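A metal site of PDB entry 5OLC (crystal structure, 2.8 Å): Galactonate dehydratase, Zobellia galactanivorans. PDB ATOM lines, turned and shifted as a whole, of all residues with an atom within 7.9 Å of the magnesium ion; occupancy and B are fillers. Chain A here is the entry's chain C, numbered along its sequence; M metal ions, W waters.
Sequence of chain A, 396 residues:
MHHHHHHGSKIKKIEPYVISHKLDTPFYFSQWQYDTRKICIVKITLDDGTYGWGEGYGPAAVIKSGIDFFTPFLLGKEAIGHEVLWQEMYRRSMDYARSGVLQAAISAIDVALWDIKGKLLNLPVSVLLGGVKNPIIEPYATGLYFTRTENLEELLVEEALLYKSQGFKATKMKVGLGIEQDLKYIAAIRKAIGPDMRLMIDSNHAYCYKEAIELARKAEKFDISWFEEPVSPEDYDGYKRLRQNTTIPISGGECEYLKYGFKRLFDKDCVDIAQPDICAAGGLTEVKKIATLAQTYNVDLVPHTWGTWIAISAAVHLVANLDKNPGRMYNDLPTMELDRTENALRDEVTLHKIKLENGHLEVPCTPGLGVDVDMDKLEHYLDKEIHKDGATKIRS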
ATOM      1  N   TYR A  57      16.174  18.635 -16.018  1.00  0.00           N
ATOM      2  CA  TYR A  57      14.699  18.644 -16.081  1.00  0.00           C
ATOM      3  C   TYR A  57      14.161  17.288 -16.496  1.00  0.00           C
ATOM      4  O   TYR A  57      14.586  16.743 -17.512  1.00  0.00           O
ATOM      5  CB  TYR A  57      14.174  19.744 -17.014  1.00  0.00           C
ATOM      6  CG  TYR A  57      12.659  19.800 -17.137  1.00  0.00           C
ATOM      7  CD1 TYR A  57      11.881  20.511 -16.221  1.00  0.00           C
ATOM      8  CD2 TYR A  57      12.009  19.208 -18.220  1.00  0.00           C
ATOM      9  CE1 TYR A  57      10.498  20.592 -16.360  1.00  0.00           C
ATOM     10  CE2 TYR A  57      10.621  19.281 -18.369  1.00  0.00           C
ATOM     11  CZ  TYR A  57       9.872  19.980 -17.433  1.00  0.00           C
ATOM     12  OH  TYR A  57       8.506  20.050 -17.592  1.00  0.00           O
ATOM     13  N   TYR A 140       6.899  36.048 -18.110  1.00  0.00           N
ATOM     14  CA  TYR A 140       5.463  35.761 -17.996  1.00  0.00           C
ATOM     15  C   TYR A 140       5.186  34.847 -16.793  1.00  0.00           C
ATOM     16  O   TYR A 140       6.044  34.055 -16.399  1.00  0.00           O
ATOM     17  CB  TYR A 140       4.863  35.221 -19.307  1.00  0.00           C
ATOM     18  CG  TYR A 140       5.473  33.944 -19.841  1.00  0.00           C
ATOM     19  CD1 TYR A 140       6.563  33.976 -20.706  1.00  0.00           C
ATOM     20  CD2 TYR A 140       4.900  32.711 -19.570  1.00  0.00           C
ATOM     21  CE1 TYR A 140       7.109  32.812 -21.227  1.00  0.00           C
ATOM     22  CE2 TYR A 140       5.441  31.525 -20.083  1.00  0.00           C
ATOM     23  CZ  TYR A 140       6.541  31.585 -20.916  1.00  0.00           C
ATOM     24  OH  TYR A 140       7.085  30.435 -21.426  1.00  0.00           O
ATOM     25  N   THR A 142       3.233  31.781 -15.085  1.00  0.00           N
ATOM     26  CA  THR A 142       2.553  30.517 -15.419  1.00  0.00           C
ATOM     27  C   THR A 142       1.618  30.092 -14.258  1.00  0.00           C
ATOM     28  O   THR A 142       2.071  30.022 -13.110  1.00  0.00           O
ATOM     29  CB  THR A 142       3.544  29.419 -15.827  1.00  0.00           C
ATOM     30  OG1 THR A 142       4.427  29.121 -14.749  1.00  0.00           O
ATOM     31  CG2 THR A 142       4.326  29.778 -17.064  1.00  0.00           C
ATOM     32  N   LYS A 172       0.699  32.945 -18.795  1.00  0.00           N
ATOM     33  CA  LYS A 172       0.463  31.690 -19.509  1.00  0.00           C
ATOM     34  C   LYS A 172      -0.461  30.747 -18.722  1.00  0.00           C
ATOM     35  O   LYS A 172      -0.117  30.308 -17.613  1.00  0.00           O
ATOM     36  CB  LYS A 172       1.780  30.996 -19.891  1.00  0.00           C
ATOM     37  CG  LYS A 172       1.606  29.823 -20.839  1.00  0.00           C
ATOM     38  CD  LYS A 172       2.902  29.099 -21.103  1.00  0.00           C
ATOM     39  CE  LYS A 172       3.131  27.961 -20.158  1.00  0.00           C
ATOM     40  NZ  LYS A 172       4.480  27.369 -20.335  1.00  0.00           N
ATOM     41  N   MET A 173      -1.609  30.435 -19.324  1.00  0.00           N
ATOM     42  CA  MET A 173      -2.629  29.568 -18.746  1.00  0.00           C
ATOM     43  C   MET A 173      -2.626  28.145 -19.331  1.00  0.00           C
ATOM     44  O   MET A 173      -2.321  27.970 -20.514  1.00  0.00           O
ATOM     45  CB  MET A 173      -4.019  30.208 -18.829  1.00  0.00           C
ATOM     46  CG  MET A 173      -4.493  30.451 -20.240  1.00  0.00           C
ATOM     47  SD  MET A 173      -6.216  30.956 -20.297  1.00  0.00           S
ATOM     48  CE  MET A 173      -7.043  29.408 -19.756  1.00  0.00           C
ATOM     49  N   LYS A 174      -2.968  27.153 -18.503  1.00  0.00           N
ATOM     50  CA  LYS A 174      -3.016  25.760 -18.928  1.00  0.00           C
ATOM     51  C   LYS A 174      -4.402  25.384 -19.418  1.00  0.00           C
ATOM     52  O   LYS A 174      -5.393  25.694 -18.766  1.00  0.00           O
ATOM     53  CB  LYS A 174      -2.506  24.801 -17.849  1.00  0.00           C
ATOM     54  CG  LYS A 174      -1.205  24.069 -18.243  1.00  0.00           C
ATOM     55  CD  LYS A 174       0.050  24.732 -17.673  1.00  0.00           C
ATOM     56  CE  LYS A 174       1.335  23.978 -17.918  1.00  0.00           C
ATOM     57  NZ  LYS A 174       2.476  24.929 -18.109  1.00  0.00           N
ATOM     58  N   ILE A 201      -1.837  30.301 -24.201  1.00  0.00           N
ATOM     59  CA  ILE A 201      -2.471  29.021 -23.844  1.00  0.00           C
ATOM     60  C   ILE A 201      -1.496  27.833 -24.036  1.00  0.00           C
ATOM     61  O   ILE A 201      -0.731  27.807 -25.001  1.00  0.00           O
ATOM     62  CB  ILE A 201      -3.843  28.813 -24.546  1.00  0.00           C
ATOM     63  CG1 ILE A 201      -3.736  28.878 -26.092  1.00  0.00           C
ATOM     64  CG2 ILE A 201      -4.862  29.824 -24.032  1.00  0.00           C
ATOM     65  CD1 ILE A 201      -4.835  28.158 -26.871  1.00  0.00           C
ATOM     66  N   ASP A 202      -1.504  26.878 -23.078  1.00  0.00           N
ATOM     67  CA  ASP A 202      -0.635  25.697 -23.102  1.00  0.00           C
ATOM     68  C   ASP A 202      -1.454  24.410 -22.959  1.00  0.00           C
ATOM     69  O   ASP A 202      -2.031  24.157 -21.903  1.00  0.00           O
ATOM     70  CB  ASP A 202       0.447  25.802 -22.011  1.00  0.00           C
ATOM     71  CG  ASP A 202       1.432  24.639 -21.931  1.00  0.00           C
ATOM     72  OD1 ASP A 202       1.536  23.860 -22.915  1.00  0.00           O
ATOM     73  OD2 ASP A 202       2.129  24.527 -20.899  1.00  0.00           O
ATOM     74  N   SER A 203      -1.501  23.601 -24.019  1.00  0.00           N
ATOM     75  CA  SER A 203      -2.255  22.352 -24.073  1.00  0.00           C
ATOM     76  C   SER A 203      -1.579  21.222 -23.328  1.00  0.00           C
ATOM     77  O   SER A 203      -2.267  20.470 -22.637  1.00  0.00           O
ATOM     78  CB  SER A 203      -2.496  21.934 -25.519  1.00  0.00           C
ATOM     79  OG  SER A 203      -2.893  20.575 -25.621  1.00  0.00           O
ATOM     80  N   ASN A 204      -0.233  21.098 -23.463  1.00  0.00           N
ATOM     81  CA  ASN A 204       0.621  20.021 -22.931  1.00  0.00           C
ATOM     82  C   ASN A 204       0.310  18.767 -23.737  1.00  0.00           C
ATOM     83  O   ASN A 204       0.011  17.720 -23.161  1.00  0.00           O
ATOM     84  CB  ASN A 204       0.439  19.762 -21.415  1.00  0.00           C
ATOM     85  CG  ASN A 204       0.359  21.000 -20.570  1.00  0.00           C
ATOM     86  OD1 ASN A 204       1.364  21.604 -20.219  1.00  0.00           O
ATOM     87  ND2 ASN A 204      -0.855  21.386 -20.200  1.00  0.00           N
ATOM     88  N   HIS A 205       0.324  18.906 -25.102  1.00  0.00           N
ATOM     89  CA  HIS A 205       0.027  17.870 -26.117  1.00  0.00           C
ATOM     90  C   HIS A 205      -1.239  17.032 -25.774  1.00  0.00           C
ATOM     91  O   HIS A 205      -1.382  15.891 -26.230  1.00  0.00           O
ATOM     92  CB  HIS A 205       1.247  16.968 -26.431  1.00  0.00           C
ATOM     93  CG  HIS A 205       2.277  16.924 -25.348  1.00  0.00           C
ATOM     94  ND1 HIS A 205       3.225  17.916 -25.220  1.00  0.00           N
ATOM     95  CD2 HIS A 205       2.415  16.042 -24.333  1.00  0.00           C
ATOM     96  CE1 HIS A 205       3.932  17.603 -24.147  1.00  0.00           C
ATOM     97  NE2 HIS A 205       3.479  16.487 -23.588  1.00  0.00           N
ATOM     98  N   TRP A 226       0.325  33.263 -28.022  1.00  0.00           N
ATOM     99  CA  TRP A 226       0.819  32.017 -28.608  1.00  0.00           C
ATOM    100  C   TRP A 226       0.139  30.770 -28.009  1.00  0.00           C
ATOM    101  O   TRP A 226      -0.376  30.807 -26.888  1.00  0.00           O
ATOM    102  CB  TRP A 226       2.370  31.877 -28.598  1.00  0.00           C
ATOM    103  CG  TRP A 226       3.010  31.475 -27.310  1.00  0.00           C
ATOM    104  CD1 TRP A 226       2.938  30.263 -26.696  1.00  0.00           C
ATOM    105  CD2 TRP A 226       3.969  32.243 -26.562  1.00  0.00           C
ATOM    106  NE1 TRP A 226       3.721  30.242 -25.568  1.00  0.00           N
ATOM    107  CE2 TRP A 226       4.357  31.453 -25.458  1.00  0.00           C
ATOM    108  CE3 TRP A 226       4.472  33.546 -26.682  1.00  0.00           C
ATOM    109  CZ2 TRP A 226       5.256  31.910 -24.485  1.00  0.00           C
ATOM    110  CZ3 TRP A 226       5.365  33.996 -25.719  1.00  0.00           C
ATOM    111  CH2 TRP A 226       5.757  33.179 -24.646  1.00  0.00           C
ATOM    112  N   PHE A 227       0.185  29.668 -28.780  1.00  0.00           N
ATOM    113  CA  PHE A 227      -0.318  28.360 -28.380  1.00  0.00           C
ATOM    114  C   PHE A 227       0.888  27.400 -28.206  1.00  0.00           C
ATOM    115  O   PHE A 227       1.561  27.027 -29.169  1.00  0.00           O
ATOM    116  CB  PHE A 227      -1.357  27.837 -29.399  1.00  0.00           C
ATOM    117  CG  PHE A 227      -2.194  26.636 -29.003  1.00  0.00           C
ATOM    118  CD1 PHE A 227      -2.040  26.032 -27.765  1.00  0.00           C
ATOM    119  CD2 PHE A 227      -3.138  26.119 -29.879  1.00  0.00           C
ATOM    120  CE1 PHE A 227      -2.811  24.935 -27.402  1.00  0.00           C
ATOM    121  CE2 PHE A 227      -3.907  25.007 -29.517  1.00  0.00           C
ATOM    122  CZ  PHE A 227      -3.741  24.420 -28.288  1.00  0.00           C
ATOM    123  N   GLU A 228       1.158  27.058 -26.924  1.00  0.00           N
ATOM    124  CA  GLU A 228       2.252  26.194 -26.497  1.00  0.00           C
ATOM    125  C   GLU A 228       1.860  24.726 -26.533  1.00  0.00           C
ATOM    126  O   GLU A 228       0.767  24.354 -26.085  1.00  0.00           O
ATOM    127  CB  GLU A 228       2.752  26.604 -25.095  1.00  0.00           C
ATOM    128  CG  GLU A 228       4.209  26.244 -24.868  1.00  0.00           C
ATOM    129  CD  GLU A 228       4.762  26.641 -23.515  1.00  0.00           C
ATOM    130  OE1 GLU A 228       4.887  27.859 -23.257  1.00  0.00           O
ATOM    131  OE2 GLU A 228       5.124  25.740 -22.727  1.00  0.00           O
ATOM    132  N   GLU A 229       2.772  23.888 -27.081  1.00  0.00           N
ATOM    133  CA  GLU A 229       2.638  22.445 -27.270  1.00  0.00           C
ATOM    134  C   GLU A 229       1.183  22.028 -27.663  1.00  0.00           C
ATOM    135  O   GLU A 229       0.535  21.278 -26.911  1.00  0.00           O
ATOM    136  CB  GLU A 229       3.179  21.704 -26.020  1.00  0.00           C
ATOM    137  CG  GLU A 229       4.690  21.788 -25.861  1.00  0.00           C
ATOM    138  CD  GLU A 229       5.511  20.755 -26.610  1.00  0.00           C
ATOM    139  OE1 GLU A 229       5.417  19.551 -26.277  1.00  0.00           O
ATOM    140  OE2 GLU A 229       6.320  21.158 -27.484  1.00  0.00           O
ATOM    141  N   PRO A 230       0.624  22.533 -28.795  1.00  0.00           N
ATOM    142  CA  PRO A 230      -0.774  22.221 -29.151  1.00  0.00           C
ATOM    143  C   PRO A 230      -1.102  20.759 -29.456  1.00  0.00           C
ATOM    144  O   PRO A 230      -2.209  20.306 -29.142  1.00  0.00           O
ATOM    145  CB  PRO A 230      -1.028  23.104 -30.369  1.00  0.00           C
ATOM    146  CG  PRO A 230       0.310  23.320 -30.959  1.00  0.00           C
ATOM    147  CD  PRO A 230       1.214  23.456 -29.790  1.00  0.00           C
ATOM    148  N   SER A 251       3.870  27.595 -30.612  1.00  0.00           N
ATOM    149  CA  SER A 251       5.041  27.329 -29.776  1.00  0.00           C
ATOM    150  C   SER A 251       5.246  25.829 -29.609  1.00  0.00           C
ATOM    151  O   SER A 251       4.271  25.077 -29.596  1.00  0.00           O
ATOM    152  CB  SER A 251       4.827  27.928 -28.402  1.00  0.00           C
ATOM    153  OG  SER A 251       5.556  29.127 -28.250  1.00  0.00           O
ATOM    154  N   GLY A 252       6.496  25.431 -29.448  1.00  0.00           N
ATOM    155  CA  GLY A 252       6.830  24.031 -29.254  1.00  0.00           C
ATOM    156  C   GLY A 252       8.325  23.754 -29.202  1.00  0.00           C
ATOM    157  O   GLY A 252       9.135  24.561 -29.657  1.00  0.00           O
ATOM    158  N   GLU A 254       9.507  21.934 -26.164  1.00  0.00           N
ATOM    159  CA  GLU A 254       9.743  21.547 -24.754  1.00  0.00           C
ATOM    160  C   GLU A 254      10.455  20.197 -24.780  1.00  0.00           C
ATOM    161  O   GLU A 254      11.562  20.066 -24.279  1.00  0.00           O
ATOM    162  CB  GLU A 254       8.409  21.332 -24.014  1.00  0.00           C
ATOM    163  CG  GLU A 254       7.663  22.566 -23.554  1.00  0.00           C
ATOM    164  CD  GLU A 254       6.539  22.211 -22.585  1.00  0.00           C
ATOM    165  OE1 GLU A 254       5.444  22.792 -22.734  1.00  0.00           O
ATOM    166  OE2 GLU A 254       6.751  21.344 -21.699  1.00  0.00           O
ATOM    167  N   GLN A 275      10.909  26.527 -28.005  1.00  0.00           N
ATOM    168  CA  GLN A 275      11.017  26.579 -26.548  1.00  0.00           C
ATOM    169  C   GLN A 275      11.896  25.467 -25.968  1.00  0.00           C
ATOM    170  O   GLN A 275      11.373  24.586 -25.279  1.00  0.00           O
ATOM    171  CB  GLN A 275       9.610  26.614 -25.878  1.00  0.00           C
ATOM    172  CG  GLN A 275       8.780  27.818 -26.293  1.00  0.00           C
ATOM    173  CD  GLN A 275       7.735  28.250 -25.306  1.00  0.00           C
ATOM    174  OE1 GLN A 275       6.587  28.506 -25.681  1.00  0.00           O
ATOM    175  NE2 GLN A 275       8.116  28.444 -24.047  1.00  0.00           N
ATOM    176  N   HIS A 304      12.092  27.145 -22.252  1.00  0.00           N
ATOM    177  CA  HIS A 304      11.147  26.564 -21.319  1.00  0.00           C
ATOM    178  C   HIS A 304      11.865  26.491 -19.964  1.00  0.00           C
ATOM    179  O   HIS A 304      13.040  26.096 -19.925  1.00  0.00           O
ATOM    180  CB  HIS A 304      10.715  25.167 -21.783  1.00  0.00           C
ATOM    181  CG  HIS A 304       9.733  24.490 -20.865  1.00  0.00           C
ATOM    182  ND1 HIS A 304      10.107  23.425 -20.054  1.00  0.00           N
ATOM    183  CD2 HIS A 304       8.414  24.728 -20.675  1.00  0.00           C
ATOM    184  CE1 HIS A 304       9.019  23.073 -19.385  1.00  0.00           C
ATOM    185  NE2 HIS A 304       7.979  23.826 -19.725  1.00  0.00           N
ATOM    186  N   GLU A 337      10.131  32.007 -19.152  1.00  0.00           N
ATOM    187  CA  GLU A 337       9.165  31.321 -18.294  1.00  0.00           C
ATOM    188  C   GLU A 337       9.473  31.482 -16.818  1.00  0.00           C
ATOM    189  O   GLU A 337      10.461  30.937 -16.319  1.00  0.00           O
ATOM    190  CB  GLU A 337       9.007  29.833 -18.676  1.00  0.00           C
ATOM    191  CG  GLU A 337       7.774  29.181 -18.083  1.00  0.00           C
ATOM    192  CD  GLU A 337       7.299  27.877 -18.694  1.00  0.00           C
ATOM    193  OE1 GLU A 337       7.487  27.681 -19.910  1.00  0.00           O
ATOM    194  OE2 GLU A 337       6.679  27.082 -17.954  1.00  0.00           O
HETATM  195 MG    MG M   1       4.138  24.086 -22.154  1.00  0.00          MG
HETATM  196  O   HOH W   1       3.504  21.223 -21.819  1.00  0.00           O
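NZ of Lys 172 touches the magnesium ion (3.8 Å).
Of the 22 residues printed, 4 come within 4 Å of the magnesium ion.
Along chain A the residues within 4 Å of the magnesium ion span positions 172 to 254.
The nearest printed residue that does not touch the magnesium ion is Asn 204 (4.2 Å).
The magnesium ion is bound by the side-chain carboxylate (OE1) of Glu 254 (1.9 Å), the side-chain carboxylate (OE2) of Glu 228 (2.0 Å) and the side-chain carboxylate (OD2) of Asp 202 (2.4 Å).
Slightly farther from the magnesium ion lies the side-chain carboxylate (OD1) of Asp 202 (2.7 Å).
The side-chain carboxylate of Glu 254 lies within hydrogen-bond range of a ring nitrogen (NE2) of His 304 (3.4 Å).
The backbone NH of Asp 202 lies within hydrogen-bond range of the backbone carbonyl oxygen of Met 173, 2.9 Å away.
OD1 of Asp 202 sits at hydrogen-bond distance from N of Asn 204, 3.3 Å away.
The side-chain amino group of Lys 174 sits close to the side-chain carboxylate of Asp 202 (2.8 Å).
The backbone NH (N) of Glu 254 lies within hydrogen-bond range of the backbone carbonyl oxygen (O) of Gln 275, at 3.4 Å.
The backbone NH (N) of Ser 203 sits at hydrogen-bond distance from the backbone carbonyl oxygen (O) of Glu 228, at 3.2 Å.
The side-chain carboxylate (OD2) of Asp 202 lies close to the side-chain amino group (NZ) of Lys 172, at 3.7 Å.
The side-chain carboxylate (OE1) of Glu 228 lies within salt-bridge range of the side-chain amino group (NZ) of Lys 172, at 3.0 Å.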
